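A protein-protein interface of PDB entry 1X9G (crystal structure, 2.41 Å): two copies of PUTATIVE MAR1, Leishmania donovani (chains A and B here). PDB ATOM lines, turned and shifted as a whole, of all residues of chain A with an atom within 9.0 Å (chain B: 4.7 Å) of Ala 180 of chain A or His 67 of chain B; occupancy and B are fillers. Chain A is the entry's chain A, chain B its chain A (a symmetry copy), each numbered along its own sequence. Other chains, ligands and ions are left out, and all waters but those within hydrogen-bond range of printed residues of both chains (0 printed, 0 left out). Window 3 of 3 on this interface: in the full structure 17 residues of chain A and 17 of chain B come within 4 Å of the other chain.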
ATOM      1  N   LEU A 174      12.437 -18.387 -33.200  1.00  0.00           N
ATOM      2  CA  LEU A 174      12.108 -19.768 -32.907  1.00  0.00           C
ATOM      3  C   LEU A 174      13.224 -20.785 -33.088  1.00  0.00           C
ATOM      4  O   LEU A 174      13.157 -21.896 -32.547  1.00  0.00           O
ATOM      5  CB  LEU A 174      10.943 -20.167 -33.813  1.00  0.00           C
ATOM      6  CG  LEU A 174       9.633 -19.431 -33.519  1.00  0.00           C
ATOM      7  CD1 LEU A 174       8.448 -20.063 -34.248  1.00  0.00           C
ATOM      8  CD2 LEU A 174       9.338 -19.371 -31.982  1.00  0.00           C
ATOM      9  N   THR A 177      15.557 -20.476 -29.874  1.00  0.00           N
ATOM     10  CA  THR A 177      14.985 -20.993 -28.609  1.00  0.00           C
ATOM     11  C   THR A 177      14.344 -22.338 -28.783  1.00  0.00           C
ATOM     12  O   THR A 177      13.128 -22.412 -28.777  1.00  0.00           O
ATOM     13  CB  THR A 177      13.810 -20.119 -28.061  1.00  0.00           C
ATOM     14  OG1 THR A 177      13.235 -19.326 -29.099  1.00  0.00           O
ATOM     15  CG2 THR A 177      14.272 -19.211 -26.920  1.00  0.00           C
ATOM     16  N   LYS A 178      15.087 -23.418 -28.934  1.00  0.00           N
ATOM     17  CA  LYS A 178      14.491 -24.555 -29.631  1.00  0.00           C
ATOM     18  C   LYS A 178      13.215 -25.216 -29.009  1.00  0.00           C
ATOM     19  O   LYS A 178      12.689 -26.203 -29.544  1.00  0.00           O
ATOM     20  CB  LYS A 178      15.591 -25.551 -29.967  1.00  0.00           C
ATOM     21  CG  LYS A 178      16.660 -25.019 -30.969  1.00  0.00           C
ATOM     22  CD  LYS A 178      16.950 -26.088 -32.081  1.00  0.00           C
ATOM     23  CE  LYS A 178      18.015 -25.662 -33.089  1.00  0.00           C
ATOM     24  NZ  LYS A 178      17.611 -24.476 -33.961  1.00  0.00           N
ATOM     25  N   ASP A 179      12.687 -24.621 -27.922  1.00  0.00           N
ATOM     26  CA  ASP A 179      11.651 -25.241 -27.053  1.00  0.00           C
ATOM     27  C   ASP A 179      10.730 -24.184 -26.415  1.00  0.00           C
ATOM     28  O   ASP A 179      11.208 -23.152 -25.972  1.00  0.00           O
ATOM     29  CB  ASP A 179      12.343 -26.033 -25.939  1.00  0.00           C
ATOM     30  CG  ASP A 179      11.515 -27.221 -25.442  1.00  0.00           C
ATOM     31  OD1 ASP A 179      10.374 -27.030 -24.922  1.00  0.00           O
ATOM     32  OD2 ASP A 179      12.041 -28.361 -25.569  1.00  0.00           O
ATOM     33  N   ALA A 180       9.420 -24.434 -26.351  1.00  0.00           N
ATOM     34  CA  ALA A 180       8.489 -23.478 -25.722  1.00  0.00           C
ATOM     35  C   ALA A 180       8.570 -23.471 -24.173  1.00  0.00           C
ATOM     36  O   ALA A 180       7.912 -22.657 -23.519  1.00  0.00           O
ATOM     37  CB  ALA A 180       7.039 -23.707 -26.195  1.00  0.00           C
ATOM     38  N   MET A 181       9.370 -24.380 -23.605  1.00  0.00           N
ATOM     39  CA  MET A 181       9.645 -24.411 -22.150  1.00  0.00           C
ATOM     40  C   MET A 181      11.044 -23.889 -21.831  1.00  0.00           C
ATOM     41  O   MET A 181      11.630 -24.212 -20.802  1.00  0.00           O
ATOM     42  CB  MET A 181       9.432 -25.821 -21.582  1.00  0.00           C
ATOM     43  CG  MET A 181       7.953 -26.240 -21.519  1.00  0.00           C
ATOM     44  SD  MET A 181       6.932 -25.365 -20.273  1.00  0.00           S
ATOM     45  CE  MET A 181       6.178 -24.015 -21.210  1.00  0.00           C
ATOM     46  N   ASP A 182      11.562 -23.072 -22.736  1.00  0.00           N
ATOM     47  CA  ASP A 182      12.898 -22.502 -22.618  1.00  0.00           C
ATOM     48  C   ASP A 182      12.834 -21.360 -21.616  1.00  0.00           C
ATOM     49  O   ASP A 182      11.855 -20.615 -21.627  1.00  0.00           O
ATOM     50  CB  ASP A 182      13.354 -21.964 -23.984  1.00  0.00           C
ATOM     51  CG  ASP A 182      14.811 -21.596 -23.995  1.00  0.00           C
ATOM     52  OD1 ASP A 182      15.644 -22.498 -24.228  1.00  0.00           O
ATOM     53  OD2 ASP A 182      15.132 -20.419 -23.747  1.00  0.00           O
ATOM     54  N   PRO A 183      13.883 -21.197 -20.770  1.00  0.00           N
ATOM     55  CA  PRO A 183      13.822 -20.174 -19.707  1.00  0.00           C
ATOM     56  C   PRO A 183      13.572 -18.805 -20.314  1.00  0.00           C
ATOM     57  O   PRO A 183      12.986 -17.912 -19.666  1.00  0.00           O
ATOM     58  CB  PRO A 183      15.216 -20.234 -19.071  1.00  0.00           C
ATOM     59  CG  PRO A 183      15.700 -21.595 -19.338  1.00  0.00           C
ATOM     60  CD  PRO A 183      15.159 -21.937 -20.719  1.00  0.00           C
ATOM     61  N   ASN A 184      13.984 -18.644 -21.569  1.00  0.00           N
ATOM     62  CA  ASN A 184      13.812 -17.344 -22.201  1.00  0.00           C
ATOM     63  C   ASN A 184      12.580 -17.167 -23.097  1.00  0.00           C
ATOM     64  O   ASN A 184      12.329 -16.069 -23.593  1.00  0.00           O
ATOM     65  CB  ASN A 184      15.115 -16.848 -22.822  1.00  0.00           C
ATOM     66  CG  ASN A 184      16.034 -16.279 -21.784  1.00  0.00           C
ATOM     67  OD1 ASN A 184      15.665 -15.351 -21.053  1.00  0.00           O
ATOM     68  ND2 ASN A 184      17.227 -16.836 -21.686  1.00  0.00           N
ATOM     69  N   PHE A 185      11.782 -18.226 -23.198  1.00  0.00           N
ATOM     70  CA  PHE A 185      10.663 -18.231 -24.099  1.00  0.00           C
ATOM     71  C   PHE A 185       9.581 -17.160 -23.900  1.00  0.00           C
ATOM     72  O   PHE A 185       9.231 -16.498 -24.864  1.00  0.00           O
ATOM     73  CB  PHE A 185      10.041 -19.626 -24.280  1.00  0.00           C
ATOM     74  CG  PHE A 185       8.949 -19.629 -25.293  1.00  0.00           C
ATOM     75  CD1 PHE A 185       7.634 -19.857 -24.920  1.00  0.00           C
ATOM     76  CD2 PHE A 185       9.227 -19.276 -26.629  1.00  0.00           C
ATOM     77  CE1 PHE A 185       6.601 -19.807 -25.890  1.00  0.00           C
ATOM     78  CE2 PHE A 185       8.224 -19.203 -27.585  1.00  0.00           C
ATOM     79  CZ  PHE A 185       6.907 -19.473 -27.225  1.00  0.00           C
ATOM     80  N   LYS A 186       9.036 -17.025 -22.702  1.00  0.00           N
ATOM     81  CA  LYS A 186       8.030 -16.003 -22.347  1.00  0.00           C
ATOM     82  C   LYS A 186       8.448 -14.605 -22.791  1.00  0.00           C
ATOM     83  O   LYS A 186       7.631 -13.826 -23.298  1.00  0.00           O
ATOM     84  CB  LYS A 186       7.839 -15.989 -20.810  1.00  0.00           C
ATOM     85  CG  LYS A 186       6.579 -15.239 -20.230  1.00  0.00           C
ATOM     86  CD  LYS A 186       5.448 -16.241 -19.817  1.00  0.00           C
ATOM     87  CE  LYS A 186       4.431 -15.609 -18.834  1.00  0.00           C
ATOM     88  NZ  LYS A 186       4.859 -15.682 -17.367  1.00  0.00           N
ATOM     89  N   ARG A 187       9.720 -14.288 -22.574  1.00  0.00           N
ATOM     90  CA  ARG A 187      10.268 -13.011 -22.995  1.00  0.00           C
ATOM     91  C   ARG A 187      10.282 -12.878 -24.521  1.00  0.00           C
ATOM     92  O   ARG A 187       9.827 -11.872 -25.063  1.00  0.00           O
ATOM     93  CB  ARG A 187      11.681 -12.820 -22.433  1.00  0.00           C
ATOM     94  CG  ARG A 187      11.777 -12.082 -21.089  1.00  0.00           C
ATOM     95  CD  ARG A 187      13.221 -12.120 -20.591  1.00  0.00           C
ATOM     96  NE  ARG A 187      13.921 -10.846 -20.790  1.00  0.00           N
ATOM     97  CZ  ARG A 187      15.124 -10.538 -20.285  1.00  0.00           C
ATOM     98  NH1 ARG A 187      15.806 -11.431 -19.561  1.00  0.00           N
ATOM     99  NH2 ARG A 187      15.663  -9.338 -20.521  1.00  0.00           N
ATOM    100  N   SER A 189       8.735 -14.904 -26.760  1.00  0.00           N
ATOM    101  CA  SER A 189       7.354 -15.060 -27.232  1.00  0.00           C
ATOM    102  C   SER A 189       6.658 -13.699 -27.368  1.00  0.00           C
ATOM    103  O   SER A 189       5.887 -13.472 -28.298  1.00  0.00           O
ATOM    104  CB  SER A 189       6.584 -15.973 -26.258  1.00  0.00           C
ATOM    105  OG  SER A 189       5.222 -16.136 -26.608  1.00  0.00           O
ATOM    106  N   ASP B  27       1.131 -30.781 -35.511  1.00  0.00           N
ATOM    107  CA  ASP B  27       0.473 -29.641 -34.824  1.00  0.00           C
ATOM    108  C   ASP B  27      -0.843 -29.075 -35.406  1.00  0.00           C
ATOM    109  O   ASP B  27      -1.166 -27.903 -35.230  1.00  0.00           O
ATOM    110  CB  ASP B  27       1.482 -28.523 -34.551  1.00  0.00           C
ATOM    111  CG  ASP B  27       2.694 -29.003 -33.768  1.00  0.00           C
ATOM    112  OD1 ASP B  27       3.642 -28.177 -33.617  1.00  0.00           O
ATOM    113  OD2 ASP B  27       2.712 -30.171 -33.289  1.00  0.00           O
ATOM    114  N   GLN B  29      -3.865 -28.240 -34.644  1.00  0.00           N
ATOM    115  CA  GLN B  29      -4.652 -28.060 -33.420  1.00  0.00           C
ATOM    116  C   GLN B  29      -5.583 -26.846 -33.503  1.00  0.00           C
ATOM    117  O   GLN B  29      -5.512 -26.046 -34.452  1.00  0.00           O
ATOM    118  CB  GLN B  29      -3.706 -27.944 -32.216  1.00  0.00           C
ATOM    119  CG  GLN B  29      -2.478 -28.798 -32.410  1.00  0.00           C
ATOM    120  CD  GLN B  29      -1.465 -28.674 -31.333  1.00  0.00           C
ATOM    121  OE1 GLN B  29      -0.294 -28.993 -31.539  1.00  0.00           O
ATOM    122  NE2 GLN B  29      -1.897 -28.233 -30.150  1.00  0.00           N
ATOM    123  N   THR B  65       1.702 -35.284 -33.561  1.00  0.00           N
ATOM    124  CA  THR B  65       2.215 -34.527 -32.415  1.00  0.00           C
ATOM    125  C   THR B  65       1.218 -33.409 -32.124  1.00  0.00           C
ATOM    126  O   THR B  65       0.663 -32.799 -33.061  1.00  0.00           O
ATOM    127  CB  THR B  65       3.605 -33.905 -32.679  1.00  0.00           C
ATOM    128  OG1 THR B  65       3.460 -32.908 -33.679  1.00  0.00           O
ATOM    129  CG2 THR B  65       4.582 -34.914 -33.174  1.00  0.00           C
ATOM    130  N   GLU B  66       0.968 -33.158 -30.833  1.00  0.00           N
ATOM    131  CA  GLU B  66       0.254 -31.959 -30.419  1.00  0.00           C
ATOM    132  C   GLU B  66       1.229 -31.175 -29.581  1.00  0.00           C
ATOM    133  O   GLU B  66       1.862 -31.721 -28.673  1.00  0.00           O
ATOM    134  CB  GLU B  66      -0.977 -32.235 -29.558  1.00  0.00           C
ATOM    135  CG  GLU B  66      -1.712 -33.548 -29.751  1.00  0.00           C
ATOM    136  CD  GLU B  66      -3.089 -33.518 -29.117  1.00  0.00           C
ATOM    137  OE1 GLU B  66      -3.187 -33.543 -27.865  1.00  0.00           O
ATOM    138  OE2 GLU B  66      -4.078 -33.449 -29.872  1.00  0.00           O
ATOM    139  N   HIS B  67       1.304 -29.885 -29.875  1.00  0.00           N
ATOM    140  CA  HIS B  67       2.219 -28.963 -29.242  1.00  0.00           C
ATOM    141  C   HIS B  67       1.477 -28.180 -28.180  1.00  0.00           C
ATOM    142  O   HIS B  67       0.422 -27.620 -28.461  1.00  0.00           O
ATOM    143  CB  HIS B  67       2.717 -27.975 -30.294  1.00  0.00           C
ATOM    144  CG  HIS B  67       3.773 -27.059 -29.794  1.00  0.00           C
ATOM    145  ND1 HIS B  67       5.107 -27.407 -29.781  1.00  0.00           N
ATOM    146  CD2 HIS B  67       3.694 -25.814 -29.267  1.00  0.00           C
ATOM    147  CE1 HIS B  67       5.810 -26.404 -29.290  1.00  0.00           C
ATOM    148  NE2 HIS B  67       4.976 -25.431 -28.959  1.00  0.00           N
ATOM    149  N   TYR B  68       2.056 -28.126 -26.978  1.00  0.00           N
ATOM    150  CA  TYR B  68       1.418 -27.570 -25.767  1.00  0.00           C
ATOM    151  C   TYR B  68      -0.123 -27.633 -25.820  1.00  0.00           C
ATOM    152  O   TYR B  68      -0.788 -26.600 -25.877  1.00  0.00           O
ATOM    153  CB  TYR B  68       1.920 -26.154 -25.535  1.00  0.00           C
ATOM    154  CG  TYR B  68       1.660 -25.592 -24.158  1.00  0.00           C
ATOM    155  CD1 TYR B  68       0.813 -24.478 -23.986  1.00  0.00           C
ATOM    156  CD2 TYR B  68       2.264 -26.151 -23.024  1.00  0.00           C
ATOM    157  CE1 TYR B  68       0.564 -23.946 -22.724  1.00  0.00           C
ATOM    158  CE2 TYR B  68       2.011 -25.625 -21.749  1.00  0.00           C
ATOM    159  CZ  TYR B  68       1.166 -24.521 -21.611  1.00  0.00           C
ATOM    160  OH  TYR B  68       0.935 -23.983 -20.361  1.00  0.00           O
ATOM    161  N   PRO B  69      -0.684 -28.867 -25.817  1.00  0.00           N
ATOM    162  CA  PRO B  69      -2.115 -29.097 -26.114  1.00  0.00           C
ATOM    163  C   PRO B  69      -3.113 -28.295 -25.250  1.00  0.00           C
ATOM    164  O   PRO B  69      -3.900 -27.509 -25.792  1.00  0.00           O
ATOM    165  CB  PRO B  69      -2.309 -30.600 -25.884  1.00  0.00           C
ATOM    166  CG  PRO B  69      -0.971 -31.169 -25.783  1.00  0.00           C
ATOM    167  CD  PRO B  69       0.037 -30.119 -25.518  1.00  0.00           C
ATOM    168  N   GLY B  73      -5.115 -25.898 -27.501  1.00  0.00           N
ATOM    169  CA  GLY B  73      -5.282 -26.781 -28.641  1.00  0.00           C
ATOM    170  C   GLY B  73      -5.158 -28.285 -28.497  1.00  0.00           C
ATOM    171  O   GLY B  73      -4.087 -28.803 -28.195  1.00  0.00           O
ATOM    172  N   LYS B  90       4.250 -32.307 -26.987  1.00  0.00           N
ATOM    173  CA  LYS B  90       5.543 -31.716 -26.663  1.00  0.00           C
ATOM    174  C   LYS B  90       5.549 -30.224 -26.569  1.00  0.00           C
ATOM    175  O   LYS B  90       4.548 -29.557 -26.824  1.00  0.00           O
ATOM    176  CB  LYS B  90       6.603 -32.137 -27.678  1.00  0.00           C
ATOM    177  CG  LYS B  90       6.108 -32.269 -29.126  1.00  0.00           C
ATOM    178  CD  LYS B  90       5.757 -30.961 -29.804  1.00  0.00           C
ATOM    179  CE  LYS B  90       6.013 -31.114 -31.333  1.00  0.00           C
ATOM    180  NZ  LYS B  90       5.650 -29.881 -32.098  1.00  0.00           N
ATOM    181  N   THR B  91       6.705 -29.702 -26.200  1.00  0.00           N
ATOM    182  CA  THR B  91       6.906 -28.261 -26.190  1.00  0.00           C
ATOM    183  C   THR B  91       8.076 -27.856 -27.149  1.00  0.00           C
ATOM    184  O   THR B  91       8.131 -26.728 -27.649  1.00  0.00           O
ATOM    185  CB  THR B  91       7.079 -27.780 -24.747  1.00  0.00           C
ATOM    186  OG1 THR B  91       8.123 -28.545 -24.117  1.00  0.00           O
ATOM    187  CG2 THR B  91       5.763 -28.019 -23.954  1.00  0.00           C
ATOM    188  N   ARG B  92       8.971 -28.806 -27.427  1.00  0.00           N
ATOM    189  CA  ARG B  92       9.972 -28.673 -28.471  1.00  0.00           C
ATOM    190  C   ARG B  92       9.301 -28.230 -29.787  1.00  0.00           C
ATOM    191  O   ARG B  92       8.228 -28.758 -30.141  1.00  0.00           O
ATOM    192  CB  ARG B  92      10.719 -29.993 -28.611  1.00  0.00           C
ATOM    193  CG  ARG B  92      11.694 -30.089 -29.756  1.00  0.00           C
ATOM    194  CD  ARG B  92      12.937 -30.810 -29.307  1.00  0.00           C
ATOM    195  NE  ARG B  92      13.950 -29.821 -28.930  1.00  0.00           N
ATOM    196  CZ  ARG B  92      15.163 -29.721 -29.471  1.00  0.00           C
ATOM    197  NH1 ARG B  92      15.551 -30.562 -30.430  1.00  0.00           N
ATOM    198  NH2 ARG B  92      15.999 -28.781 -29.036  1.00  0.00           N
ATOM    199  N   PHE B  93       9.885 -27.231 -30.477  1.00  0.00           N
ATOM    200  CA  PHE B  93       9.274 -26.746 -31.737  1.00  0.00           C
ATOM    201  C   PHE B  93       9.353 -27.843 -32.783  1.00  0.00           C
ATOM    202  O   PHE B  93       8.370 -28.128 -33.466  1.00  0.00           O
ATOM    203  CB  PHE B  93       9.840 -25.413 -32.232  1.00  0.00           C
ATOM    204  CG  PHE B  93       9.609 -24.282 -31.294  1.00  0.00           C
ATOM    205  CD1 PHE B  93      10.646 -23.411 -30.957  1.00  0.00           C
ATOM    206  CD2 PHE B  93       8.351 -24.105 -30.692  1.00  0.00           C
ATOM    207  CE1 PHE B  93      10.429 -22.347 -30.045  1.00  0.00           C
ATOM    208  CE2 PHE B  93       8.122 -23.061 -29.761  1.00  0.00           C
ATOM    209  CZ  PHE B  93       9.176 -22.170 -29.451  1.00  0.00           C
ATOM    210  N   CYS B 120       7.633 -25.272 -36.550  1.00  0.00           N
ATOM    211  CA  CYS B 120       7.752 -26.669 -36.217  1.00  0.00           C
ATOM    212  C   CYS B 120       8.166 -27.511 -37.417  1.00  0.00           C
ATOM    213  O   CYS B 120       9.051 -28.387 -37.267  1.00  0.00           O
ATOM    214  CB  CYS B 120       6.436 -27.203 -35.604  1.00  0.00           C
ATOM    215  SG  CYS B 120       5.738 -26.223 -34.155  1.00  0.00           S
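OD1 of Asp 179 of chain A lies within hydrogen-bond range of N of Met 181 of chain A (3.1 Å).
The side-chain amide oxygen of Gln 29 of chain B is in hydrogen-bond range of the backbone NH of His 67 of chain B.
ND1 of His 67 of chain B is in hydrogen-bond range of NZ of Lys 90 of chain B.
A ring nitrogen (ND1) of His 67 of chain B is in hydrogen-bond range of the backbone carbonyl oxygen (O) of Arg 92 of chain B.
The backbone carbonyl oxygen (O) of Arg 92 of chain B lies close to the side-chain amino group (NZ) of Lys 90 of chain B (3.4 Å).
The side-chain sulfur (SG) of Cys 120 of chain B sits close to the backbone carbonyl oxygen (O) of Phe 93 of chain B, 3.3 Å away.
No position is printed for both chains.
The backbone carbonyl oxygen (O) of Lys 178 of chain A lies within hydrogen-bond range of the backbone NH (N) of Phe 93 of chain B, 3.1 Å away.
The side-chain carboxylate (OD1) of Asp 179 of chain A sits at hydrogen-bond distance from the side-chain hydroxyl (OG1) of Thr 91 of chain B (2.8 Å).
OD1 of Asp 179 of chain A sits at hydrogen-bond distance from N of Arg 92 of chain B, 3.4 Å away.
The backbone carbonyl oxygen (O) of Thr 91 of chain B lies within hydrogen-bond range of the backbone NH (N) of Ala 180 of chain A (2.9 Å).
Of the 13 printed residues of chain B, 4 touch a printed residue of chain A.
Printed residues of chain B that touch a printed residue of chain A: His 67, Thr 91, Arg 92 and Phe 93.
Hydrophobic or aromatic side chains of chain B that line the printed part of chain A: His 67 and Phe 93.
Of the 13 printed residues of chain A, 7 touch a printed residue of chain B.
Among the printed residues, 12 pairs touch across the chains.
Among the printed residues, no Asp or Glu carboxylate lies within 4 Å of a Lys or Arg side-chain nitrogen of the other chain.
Ala 180 of chain A touches just these residues of chain B: His 67, Thr 91 and Phe 93.
Of the printed residues of chain A, Thr 91 of chain B touches Asp 179, Ala 180 and Met 181.
Of the printed residues of chain B, Thr 177 of chain A touches Phe 93.
The nearest residue of chain B that does not touch Ala 180 of chain A is Arg 92 of chain B (4.5 Å).
The nearest printed residue of chain A that does not touch Arg 92 of chain B is Ala 180 of chain A (4.5 Å).
Among the printed residues, pairs that only touch across the chains: Leu 174 of chain A with Phe 93 of chain B (3.3 Å), Thr 177 of chain A with Phe 93 of chain B (3.0 Å), Lys 178 of chain A with Arg 92 of chain B (3.4 Å), Asp 179 of chain A with Phe 93 of chain B (3.8 Å), Ala 180 of chain A with His 67 of chain B (3.9 Å), Ala 180 of chain A with Phe 93 of chain B (3.8 Å), Met 181 of chain A with Thr 91 of chain B (3.5 Å) and Phe 185 of chain A with Phe 93 of chain B (3.6 Å).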
